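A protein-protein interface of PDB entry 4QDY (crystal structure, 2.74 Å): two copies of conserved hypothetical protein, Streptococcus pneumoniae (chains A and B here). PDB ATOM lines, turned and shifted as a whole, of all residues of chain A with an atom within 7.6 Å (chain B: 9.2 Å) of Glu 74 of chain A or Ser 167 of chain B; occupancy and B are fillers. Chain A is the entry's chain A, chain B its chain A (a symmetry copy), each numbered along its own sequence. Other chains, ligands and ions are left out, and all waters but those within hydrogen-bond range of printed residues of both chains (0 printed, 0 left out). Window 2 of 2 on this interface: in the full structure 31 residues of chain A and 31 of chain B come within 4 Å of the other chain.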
ATOM      1  N   LEU A  65      11.817  -9.646  18.079  1.00  0.00           N
ATOM      2  CA  LEU A  65      12.679  -8.641  18.714  1.00  0.00           C
ATOM      3  C   LEU A  65      12.571  -8.650  20.251  1.00  0.00           C
ATOM      4  O   LEU A  65      13.222  -7.826  20.901  1.00  0.00           O
ATOM      5  CB  LEU A  65      12.318  -7.227  18.205  1.00  0.00           C
ATOM      6  CG  LEU A  65      12.356  -6.934  16.699  1.00  0.00           C
ATOM      7  CD1 LEU A  65      11.957  -5.503  16.441  1.00  0.00           C
ATOM      8  CD2 LEU A  65      13.736  -7.173  16.106  1.00  0.00           C
ATOM      9  N   GLY A  71      18.887  -0.157  20.921  1.00  0.00           N
ATOM     10  CA  GLY A  71      20.010  -0.111  19.996  1.00  0.00           C
ATOM     11  C   GLY A  71      19.720  -0.742  18.651  1.00  0.00           C
ATOM     12  O   GLY A  71      18.699  -1.414  18.479  1.00  0.00           O
ATOM     13  N   THR A  72      20.629  -0.526  17.690  1.00  0.00           N
ATOM     14  CA  THR A  72      20.524  -1.044  16.327  1.00  0.00           C
ATOM     15  C   THR A  72      21.075  -2.497  16.322  1.00  0.00           C
ATOM     16  O   THR A  72      22.128  -2.765  16.905  1.00  0.00           O
ATOM     17  CB  THR A  72      21.233  -0.094  15.323  1.00  0.00           C
ATOM     18  OG1 THR A  72      21.109  -0.599  13.994  1.00  0.00           O
ATOM     19  CG2 THR A  72      22.703   0.180  15.658  1.00  0.00           C
ATOM     20  N   ILE A  73      20.313  -3.434  15.712  1.00  0.00           N
ATOM     21  CA  ILE A  73      20.631  -4.872  15.629  1.00  0.00           C
ATOM     22  C   ILE A  73      20.080  -5.467  14.307  1.00  0.00           C
ATOM     23  O   ILE A  73      19.114  -4.936  13.755  1.00  0.00           O
ATOM     24  CB  ILE A  73      20.049  -5.630  16.879  1.00  0.00           C
ATOM     25  CG1 ILE A  73      20.593  -7.085  16.998  1.00  0.00           C
ATOM     26  CG2 ILE A  73      18.501  -5.557  16.960  1.00  0.00           C
ATOM     27  CD1 ILE A  73      20.153  -7.909  18.239  1.00  0.00           C
ATOM     28  N   GLU A  74      20.695  -6.562  13.807  1.00  0.00           N
ATOM     29  CA  GLU A  74      20.188  -7.260  12.625  1.00  0.00           C
ATOM     30  C   GLU A  74      19.628  -8.609  13.089  1.00  0.00           C
ATOM     31  O   GLU A  74      20.280  -9.320  13.861  1.00  0.00           O
ATOM     32  CB  GLU A  74      21.219  -7.410  11.487  1.00  0.00           C
ATOM     33  CG  GLU A  74      22.473  -8.217  11.783  1.00  0.00           C
ATOM     34  CD  GLU A  74      23.313  -8.562  10.566  1.00  0.00           C
ATOM     35  OE1 GLU A  74      22.893  -8.240   9.430  1.00  0.00           O
ATOM     36  OE2 GLU A  74      24.372  -9.201  10.747  1.00  0.00           O
ATOM     37  N   VAL A  75      18.390  -8.923  12.671  1.00  0.00           N
ATOM     38  CA  VAL A  75      17.693 -10.137  13.103  1.00  0.00           C
ATOM     39  C   VAL A  75      17.369 -11.047  11.895  1.00  0.00           C
ATOM     40  O   VAL A  75      16.977 -10.548  10.835  1.00  0.00           O
ATOM     41  CB  VAL A  75      16.401  -9.824  13.910  1.00  0.00           C
ATOM     42  CG1 VAL A  75      16.741  -9.297  15.300  1.00  0.00           C
ATOM     43  CG2 VAL A  75      15.464  -8.865  13.168  1.00  0.00           C
ATOM     44  N   PRO A  76      17.516 -12.388  12.050  1.00  0.00           N
ATOM     45  CA  PRO A  76      17.206 -13.291  10.931  1.00  0.00           C
ATOM     46  C   PRO A  76      15.706 -13.475  10.755  1.00  0.00           C
ATOM     47  O   PRO A  76      14.977 -13.598  11.739  1.00  0.00           O
ATOM     48  CB  PRO A  76      17.879 -14.615  11.333  1.00  0.00           C
ATOM     49  CG  PRO A  76      18.622 -14.336  12.613  1.00  0.00           C
ATOM     50  CD  PRO A  76      17.972 -13.149  13.229  1.00  0.00           C
ATOM     51  N   LEU A  77      15.249 -13.483   9.498  1.00  0.00           N
ATOM     52  CA  LEU A  77      13.837 -13.671   9.172  1.00  0.00           C
ATOM     53  C   LEU A  77      13.495 -15.162   9.126  1.00  0.00           C
ATOM     54  O   LEU A  77      14.324 -15.967   8.691  1.00  0.00           O
ATOM     55  CB  LEU A  77      13.475 -13.000   7.832  1.00  0.00           C
ATOM     56  CG  LEU A  77      13.705 -11.489   7.682  1.00  0.00           C
ATOM     57  CD1 LEU A  77      13.268 -11.019   6.313  1.00  0.00           C
ATOM     58  CD2 LEU A  77      12.953 -10.691   8.735  1.00  0.00           C
ATOM     59  N   LYS A  94      18.095 -11.337   6.373  1.00  0.00           N
ATOM     60  CA  LYS A  94      18.147 -10.601   7.640  1.00  0.00           C
ATOM     61  C   LYS A  94      17.764  -9.134   7.432  1.00  0.00           C
ATOM     62  O   LYS A  94      18.040  -8.572   6.368  1.00  0.00           O
ATOM     63  CB  LYS A  94      19.547 -10.691   8.281  1.00  0.00           C
ATOM     64  CG  LYS A  94      20.003 -12.100   8.638  1.00  0.00           C
ATOM     65  CD  LYS A  94      21.397 -12.115   9.257  1.00  0.00           C
ATOM     66  CE  LYS A  94      21.826 -13.517   9.623  1.00  0.00           C
ATOM     67  NZ  LYS A  94      23.171 -13.542  10.255  1.00  0.00           N
ATOM     68  N   ILE A  95      17.134  -8.514   8.446  1.00  0.00           N
ATOM     69  CA  ILE A  95      16.745  -7.098   8.393  1.00  0.00           C
ATOM     70  C   ILE A  95      17.449  -6.349   9.535  1.00  0.00           C
ATOM     71  O   ILE A  95      17.682  -6.929  10.595  1.00  0.00           O
ATOM     72  CB  ILE A  95      15.200  -6.866   8.423  1.00  0.00           C
ATOM     73  CG1 ILE A  95      14.539  -7.359   9.746  1.00  0.00           C
ATOM     74  CG2 ILE A  95      14.530  -7.465   7.171  1.00  0.00           C
ATOM     75  CD1 ILE A  95      13.074  -6.927   9.985  1.00  0.00           C
ATOM     76  N   THR A  96      17.786  -5.068   9.311  1.00  0.00           N
ATOM     77  CA  THR A  96      18.446  -4.214  10.308  1.00  0.00           C
ATOM     78  C   THR A  96      17.376  -3.365  10.991  1.00  0.00           C
ATOM     79  O   THR A  96      16.663  -2.617  10.321  1.00  0.00           O
ATOM     80  CB  THR A  96      19.543  -3.363   9.650  1.00  0.00           C
ATOM     81  OG1 THR A  96      20.447  -4.228   8.959  1.00  0.00           O
ATOM     82  CG2 THR A  96      20.304  -2.494  10.658  1.00  0.00           C
ATOM     83  N   VAL A  97      17.253  -3.494  12.320  1.00  0.00           N
ATOM     84  CA  VAL A  97      16.236  -2.775  13.086  1.00  0.00           C
ATOM     85  C   VAL A  97      16.897  -1.887  14.155  1.00  0.00           C
ATOM     86  O   VAL A  97      17.774  -2.351  14.889  1.00  0.00           O
ATOM     87  CB  VAL A  97      15.227  -3.766  13.740  1.00  0.00           C
ATOM     88  CG1 VAL A  97      14.114  -3.025  14.469  1.00  0.00           C
ATOM     89  CG2 VAL A  97      14.627  -4.721  12.712  1.00  0.00           C
ATOM     90  N   LYS A  98      16.450  -0.615  14.239  1.00  0.00           N
ATOM     91  CA  LYS A  98      16.863   0.360  15.251  1.00  0.00           C
ATOM     92  C   LYS A  98      15.790   0.382  16.337  1.00  0.00           C
ATOM     93  O   LYS A  98      14.737   1.002  16.155  1.00  0.00           O
ATOM     94  CB  LYS A  98      17.104   1.756  14.636  1.00  0.00           C
ATOM     95  CG  LYS A  98      17.522   2.825  15.651  1.00  0.00           C
ATOM     96  CD  LYS A  98      17.561   4.219  15.043  1.00  0.00           C
ATOM     97  CE  LYS A  98      17.875   5.274  16.076  1.00  0.00           C
ATOM     98  NZ  LYS A  98      17.868   6.639  15.489  1.00  0.00           N
ATOM     99  N   SER B 131      35.201  -6.915   4.975  1.00  0.00           N
ATOM    100  CA  SER B 131      35.277  -7.965   3.953  1.00  0.00           C
ATOM    101  C   SER B 131      34.784  -7.495   2.578  1.00  0.00           C
ATOM    102  O   SER B 131      35.386  -7.870   1.571  1.00  0.00           O
ATOM    103  CB  SER B 131      34.466  -9.182   4.377  1.00  0.00           C
ATOM    104  OG  SER B 131      35.053  -9.774   5.523  1.00  0.00           O
ATOM    105  N   ASP B 132      33.712  -6.692   2.532  1.00  0.00           N
ATOM    106  CA  ASP B 132      33.169  -6.199   1.268  1.00  0.00           C
ATOM    107  C   ASP B 132      33.779  -4.840   0.926  1.00  0.00           C
ATOM    108  O   ASP B 132      33.818  -3.939   1.766  1.00  0.00           O
ATOM    109  CB  ASP B 132      31.639  -6.121   1.326  1.00  0.00           C
ATOM    110  CG  ASP B 132      31.005  -7.494   1.423  1.00  0.00           C
ATOM    111  OD1 ASP B 132      30.989  -8.063   2.536  1.00  0.00           O
ATOM    112  OD2 ASP B 132      30.579  -8.024   0.377  1.00  0.00           O
ATOM    113  N   ALA B 152      29.624   0.482   8.008  1.00  0.00           N
ATOM    114  CA  ALA B 152      29.587  -0.861   8.576  1.00  0.00           C
ATOM    115  C   ALA B 152      29.644  -0.724  10.092  1.00  0.00           C
ATOM    116  O   ALA B 152      30.695  -0.896  10.718  1.00  0.00           O
ATOM    117  CB  ALA B 152      30.730  -1.704   8.022  1.00  0.00           C
ATOM    118  N   VAL B 153      28.504  -0.305  10.663  1.00  0.00           N
ATOM    119  CA  VAL B 153      28.321   0.004  12.081  1.00  0.00           C
ATOM    120  C   VAL B 153      28.215  -1.310  12.903  1.00  0.00           C
ATOM    121  O   VAL B 153      27.460  -2.220  12.552  1.00  0.00           O
ATOM    122  CB  VAL B 153      27.083   0.935  12.302  1.00  0.00           C
ATOM    123  CG1 VAL B 153      25.806   0.393  11.655  1.00  0.00           C
ATOM    124  CG2 VAL B 153      26.864   1.273  13.775  1.00  0.00           C
ATOM    125  N   LEU B 154      29.003  -1.381  13.994  1.00  0.00           N
ATOM    126  CA  LEU B 154      29.033  -2.490  14.949  1.00  0.00           C
ATOM    127  C   LEU B 154      27.719  -2.517  15.748  1.00  0.00           C
ATOM    128  O   LEU B 154      27.326  -1.463  16.260  1.00  0.00           O
ATOM    129  CB  LEU B 154      30.259  -2.337  15.884  1.00  0.00           C
ATOM    130  CG  LEU B 154      30.419  -3.318  17.063  1.00  0.00           C
ATOM    131  CD1 LEU B 154      30.741  -4.724  16.594  1.00  0.00           C
ATOM    132  CD2 LEU B 154      31.521  -2.867  17.989  1.00  0.00           C
ATOM    133  N   PRO B 155      27.021  -3.681  15.872  1.00  0.00           N
ATOM    134  CA  PRO B 155      25.763  -3.708  16.642  1.00  0.00           C
ATOM    135  C   PRO B 155      25.968  -3.234  18.083  1.00  0.00           C
ATOM    136  O   PRO B 155      26.991  -3.544  18.697  1.00  0.00           O
ATOM    137  CB  PRO B 155      25.349  -5.182  16.593  1.00  0.00           C
ATOM    138  CG  PRO B 155      26.006  -5.718  15.376  1.00  0.00           C
ATOM    139  CD  PRO B 155      27.325  -5.016  15.317  1.00  0.00           C
ATOM    140  N   THR B 156      24.999  -2.450  18.597  1.00  0.00           N
ATOM    141  CA  THR B 156      24.988  -1.821  19.926  1.00  0.00           C
ATOM    142  C   THR B 156      25.258  -2.859  21.044  1.00  0.00           C
ATOM    143  O   THR B 156      25.970  -2.545  22.000  1.00  0.00           O
ATOM    144  CB  THR B 156      23.634  -1.122  20.148  1.00  0.00           C
ATOM    145  OG1 THR B 156      23.337  -0.300  19.018  1.00  0.00           O
ATOM    146  CG2 THR B 156      23.599  -0.276  21.415  1.00  0.00           C
ATOM    147  N   SER B 157      24.716  -4.085  20.899  1.00  0.00           N
ATOM    148  CA  SER B 157      24.854  -5.194  21.847  1.00  0.00           C
ATOM    149  C   SER B 157      26.287  -5.762  21.908  1.00  0.00           C
ATOM    150  O   SER B 157      26.645  -6.382  22.914  1.00  0.00           O
ATOM    151  CB  SER B 157      23.898  -6.321  21.466  1.00  0.00           C
ATOM    152  OG  SER B 157      24.151  -6.806  20.156  1.00  0.00           O
ATOM    153  N   GLU B 158      27.087  -5.582  20.837  1.00  0.00           N
ATOM    154  CA  GLU B 158      28.452  -6.113  20.749  1.00  0.00           C
ATOM    155  C   GLU B 158      29.471  -5.204  21.448  1.00  0.00           C
ATOM    156  O   GLU B 158      29.305  -3.982  21.467  1.00  0.00           O
ATOM    157  CB  GLU B 158      28.868  -6.302  19.280  1.00  0.00           C
ATOM    158  CG  GLU B 158      28.021  -7.280  18.473  1.00  0.00           C
ATOM    159  CD  GLU B 158      28.057  -8.750  18.853  1.00  0.00           C
ATOM    160  OE1 GLU B 158      29.006  -9.178  19.550  1.00  0.00           O
ATOM    161  OE2 GLU B 158      27.161  -9.491  18.390  1.00  0.00           O
ATOM    162  N   TYR B 164      38.088  -9.129  17.380  1.00  0.00           N
ATOM    163  CA  TYR B 164      36.697  -9.404  17.028  1.00  0.00           C
ATOM    164  C   TYR B 164      36.559  -9.728  15.541  1.00  0.00           C
ATOM    165  O   TYR B 164      37.279  -9.188  14.704  1.00  0.00           O
ATOM    166  CB  TYR B 164      35.814  -8.192  17.396  1.00  0.00           C
ATOM    167  CG  TYR B 164      34.345  -8.315  17.038  1.00  0.00           C
ATOM    168  CD1 TYR B 164      33.444  -8.920  17.908  1.00  0.00           C
ATOM    169  CD2 TYR B 164      33.845  -7.766  15.860  1.00  0.00           C
ATOM    170  CE1 TYR B 164      32.088  -9.019  17.592  1.00  0.00           C
ATOM    171  CE2 TYR B 164      32.493  -7.864  15.529  1.00  0.00           C
ATOM    172  CZ  TYR B 164      31.616  -8.487  16.402  1.00  0.00           C
ATOM    173  OH  TYR B 164      30.279  -8.573  16.086  1.00  0.00           O
ATOM    174  N   SER B 165      35.610 -10.618  15.240  1.00  0.00           N
ATOM    175  CA  SER B 165      35.209 -11.056  13.909  1.00  0.00           C
ATOM    176  C   SER B 165      33.730 -11.394  13.944  1.00  0.00           C
ATOM    177  O   SER B 165      33.311 -12.238  14.742  1.00  0.00           O
ATOM    178  CB  SER B 165      36.053 -12.234  13.433  1.00  0.00           C
ATOM    179  OG  SER B 165      35.643 -12.661  12.144  1.00  0.00           O
ATOM    180  N   GLY B 166      32.948 -10.690  13.134  1.00  0.00           N
ATOM    181  CA  GLY B 166      31.504 -10.881  13.071  1.00  0.00           C
ATOM    182  C   GLY B 166      30.796 -10.031  12.040  1.00  0.00           C
ATOM    183  O   GLY B 166      31.350  -9.045  11.541  1.00  0.00           O
ATOM    184  N   SER B 167      29.549 -10.414  11.725  1.00  0.00           N
ATOM    185  CA  SER B 167      28.708  -9.723  10.756  1.00  0.00           C
ATOM    186  C   SER B 167      28.156  -8.433  11.346  1.00  0.00           C
ATOM    187  O   SER B 167      27.593  -8.435  12.448  1.00  0.00           O
ATOM    188  CB  SER B 167      27.569 -10.624  10.291  1.00  0.00           C
ATOM    189  OG  SER B 167      28.075 -11.787   9.659  1.00  0.00           O
ATOM    190  N   VAL B 168      28.349  -7.324  10.617  1.00  0.00           N
ATOM    191  CA  VAL B 168      27.884  -5.992  11.002  1.00  0.00           C
ATOM    192  C   VAL B 168      26.972  -5.453   9.880  1.00  0.00           C
ATOM    193  O   VAL B 168      27.314  -5.607   8.703  1.00  0.00           O
ATOM    194  CB  VAL B 168      29.036  -4.998  11.344  1.00  0.00           C
ATOM    195  CG1 VAL B 168      29.800  -5.433  12.589  1.00  0.00           C
ATOM    196  CG2 VAL B 168      29.988  -4.783  10.166  1.00  0.00           C
ATOM    197  N   PRO B 169      25.814  -4.831  10.208  1.00  0.00           N
ATOM    198  CA  PRO B 169      24.936  -4.321   9.141  1.00  0.00           C
ATOM    199  C   PRO B 169      25.522  -3.114   8.408  1.00  0.00           C
ATOM    200  O   PRO B 169      26.330  -2.372   8.971  1.00  0.00           O
ATOM    201  CB  PRO B 169      23.668  -3.915   9.894  1.00  0.00           C
ATOM    202  CG  PRO B 169      24.116  -3.624  11.275  1.00  0.00           C
ATOM    203  CD  PRO B 169      25.237  -4.580  11.547  1.00  0.00           C
ATOM    204  N   LEU B 170      25.105  -2.928   7.148  1.00  0.00           N
ATOM    205  CA  LEU B 170      25.523  -1.817   6.299  1.00  0.00           C
ATOM    206  C   LEU B 170      24.394  -0.794   6.187  1.00  0.00           C
ATOM    207  O   LEU B 170      23.252  -1.170   5.919  1.00  0.00           O
ATOM    208  CB  LEU B 170      25.954  -2.314   4.907  1.00  0.00           C
ATOM    209  CG  LEU B 170      27.283  -3.080   4.834  1.00  0.00           C
ATOM    210  CD1 LEU B 170      27.370  -3.906   3.579  1.00  0.00           C
ATOM    211  CD2 LEU B 170      28.478  -2.145   4.949  1.00  0.00           C
ATOM    212  N   GLN B 171      24.717   0.493   6.422  1.00  0.00           N
ATOM    213  CA  GLN B 171      23.777   1.619   6.359  1.00  0.00           C
ATOM    214  C   GLN B 171      24.276   2.715   5.415  1.00  0.00           C
ATOM    215  O   GLN B 171      25.478   2.970   5.347  1.00  0.00           O
ATOM    216  CB  GLN B 171      23.537   2.228   7.752  1.00  0.00           C
ATOM    217  CG  GLN B 171      22.823   1.321   8.749  1.00  0.00           C
ATOM    218  CD  GLN B 171      22.634   1.979  10.099  1.00  0.00           C
ATOM    219  OE1 GLN B 171      23.482   2.734  10.592  1.00  0.00           O
ATOM    220  NE2 GLN B 171      21.541   1.645  10.762  1.00  0.00           N
ATOM    221  N   PRO B 186      25.505  -6.391  -0.533  1.00  0.00           N
ATOM    222  CA  PRO B 186      24.980  -7.213   0.578  1.00  0.00           C
ATOM    223  C   PRO B 186      24.411  -6.342   1.700  1.00  0.00           C
ATOM    224  O   PRO B 186      24.807  -5.181   1.835  1.00  0.00           O
ATOM    225  CB  PRO B 186      26.215  -8.001   1.040  1.00  0.00           C
ATOM    226  CG  PRO B 186      27.378  -7.133   0.666  1.00  0.00           C
ATOM    227  CD  PRO B 186      26.975  -6.506  -0.637  1.00  0.00           C
ATOM    228  N   PHE B 187      23.455  -6.886   2.474  1.00  0.00           N
ATOM    229  CA  PHE B 187      22.805  -6.164   3.574  1.00  0.00           C
ATOM    230  C   PHE B 187      23.756  -6.020   4.777  1.00  0.00           C
ATOM    231  O   PHE B 187      23.565  -5.114   5.593  1.00  0.00           O
ATOM    232  CB  PHE B 187      21.498  -6.854   4.003  1.00  0.00           C
ATOM    233  CG  PHE B 187      21.573  -8.342   4.254  1.00  0.00           C
ATOM    234  CD1 PHE B 187      21.942  -8.837   5.499  1.00  0.00           C
ATOM    235  CD2 PHE B 187      21.223  -9.249   3.262  1.00  0.00           C
ATOM    236  CE1 PHE B 187      22.008 -10.213   5.730  1.00  0.00           C
ATOM    237  CE2 PHE B 187      21.273 -10.625   3.498  1.00  0.00           C
ATOM    238  CZ  PHE B 187      21.665 -11.098   4.731  1.00  0.00           C
ATOM    239  N   ASP B 188      24.777  -6.894   4.877  1.00  0.00           N
ATOM    240  CA  ASP B 188      25.774  -6.856   5.944  1.00  0.00           C
ATOM    241  C   ASP B 188      27.152  -7.289   5.401  1.00  0.00           C
ATOM    242  O   ASP B 188      27.268  -7.682   4.236  1.00  0.00           O
ATOM    243  CB  ASP B 188      25.349  -7.735   7.145  1.00  0.00           C
ATOM    244  CG  ASP B 188      25.167  -9.226   6.905  1.00  0.00           C
ATOM    245  OD1 ASP B 188      25.291  -9.668   5.739  1.00  0.00           O
ATOM    246  OD2 ASP B 188      24.871  -9.948   7.879  1.00  0.00           O
ATOM    247  N   THR B 189      28.191  -7.196   6.248  1.00  0.00           N
ATOM    248  CA  THR B 189      29.573  -7.540   5.904  1.00  0.00           C
ATOM    249  C   THR B 189      30.298  -8.075   7.148  1.00  0.00           C
ATOM    250  O   THR B 189      29.861  -7.816   8.269  1.00  0.00           O
ATOM    251  CB  THR B 189      30.286  -6.302   5.312  1.00  0.00           C
ATOM    252  OG1 THR B 189      31.589  -6.670   4.861  1.00  0.00           O
ATOM    253  CG2 THR B 189      30.365  -5.127   6.292  1.00  0.00           C
ATOM    254  N   ILE B 190      31.410  -8.797   6.949  1.00  0.00           N
ATOM    255  CA  ILE B 190      32.193  -9.323   8.064  1.00  0.00           C
ATOM    256  C   ILE B 190      33.239  -8.257   8.437  1.00  0.00           C
ATOM    257  O   ILE B 190      34.025  -7.829   7.586  1.00  0.00           O
ATOM    258  CB  ILE B 190      32.835 -10.726   7.787  1.00  0.00           C
ATOM    259  CG1 ILE B 190      31.777 -11.841   7.545  1.00  0.00           C
ATOM    260  CG2 ILE B 190      33.772 -11.152   8.922  1.00  0.00           C
ATOM    261  CD1 ILE B 190      31.086 -11.908   6.142  1.00  0.00           C
ATOM    262  N   MET B 191      33.209  -7.815   9.708  1.00  0.00           N
ATOM    263  CA  MET B 191      34.144  -6.837  10.265  1.00  0.00           C
ATOM    264  C   MET B 191      35.179  -7.562  11.124  1.00  0.00           C
ATOM    265  O   MET B 191      34.802  -8.342  12.002  1.00  0.00           O
ATOM    266  CB  MET B 191      33.398  -5.761  11.079  1.00  0.00           C
ATOM    267  CG  MET B 191      34.288  -4.598  11.530  1.00  0.00           C
ATOM    268  SD  MET B 191      33.420  -3.319  12.733  1.00  0.00           S
ATOM    269  CE  MET B 191      33.226  -4.438  14.232  1.00  0.00           C
ATOM    270  N   LYS B 192      36.473  -7.316  10.864  1.00  0.00           N
ATOM    271  CA  LYS B 192      37.571  -7.913  11.623  1.00  0.00           C
ATOM    272  C   LYS B 192      38.341  -6.813  12.344  1.00  0.00           C
ATOM    273  O   LYS B 192      38.871  -5.907  11.697  1.00  0.00           O
ATOM    274  CB  LYS B 192      38.494  -8.741  10.715  1.00  0.00           C
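N of Thr 72 of chain A lies within hydrogen-bond range of OG1 of Thr 156 of chain B (3.0 Å).
The side-chain carboxylate (OE2) of Glu 74 of chain A lies close to the side-chain carboxylate (OD2) of Asp 188 of chain B (3.0 Å).
The backbone carbonyl oxygen (O) of Pro 169 of chain B lies within hydrogen-bond range of the backbone NH (N) of Val 153 of chain B.
N of Leu 170 of chain B sits at hydrogen-bond distance from O of Phe 187 of chain B (3.1 Å).
Among the printed residues, pairs that only touch across the chains: Gly 71 of chain A with Thr 156 of chain B (3.5 Å), Thr 72 of chain A with Pro 155 of chain B (3.8 Å), Thr 72 of chain A with Gln 171 of chain B (3.96 Å), Glu 74 of chain A with Ser 167 of chain B (3.5 Å), Lys 94 of chain A with Phe 187 of chain B (3.6 Å) and Thr 96 of chain A with Pro 169 of chain B (3.4 Å).
Of the printed residues of chain B, Glu 74 of chain A touches Ser 167 (3.5 Å) and Asp 188 (3.0 Å).
No residue of chain B comes within 4 Å of Ile 73 of chain A.
Of the printed residues of chain A, Asp 188 of chain B touches Glu 74 (3.0 Å).
Printed residues of chain B within 4 Å of Thr 96 of chain A: Pro 169.
Of the printed residues of chain A, Pro 155 of chain B touches Thr 72 (3.8 Å).
Printed residues of chain B within 4 Å of Thr 72 of chain A: Pro 155 (3.8 Å), Thr 156 (3.0 Å) and Gln 171 (3.96 Å).
Of the printed residues of chain A, Phe 187 of chain B touches Lys 94.
Leu 154 of chain B touches none of the printed residues of chain A.
Ser 157 of chain B touches none of the printed residues of chain A.
The nearest printed residue of chain A that does not touch Pro 169 of chain B is Glu 74 of chain A (4.4 Å).
Of the 24 printed residues of chain B, 7 touch a printed residue of chain A.
Hydrophobic or aromatic side chains of chain B within 4 Å of the printed part of chain A: Pro 169 and Phe 187.
Along chain A the printed residues that touch a printed residue of chain B span positions 71 to 96.
Among the printed residues, 8 pairs touch across the chains.
Among the printed residues, no Asp or Glu carboxylate lies within 4 Å of a Lys or Arg side-chain nitrogen of the other chain.
No position is printed for both chains.
Of the 8 pairs that touch across the chains among the printed residues, none has its exchanged pair printed and touching as well.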
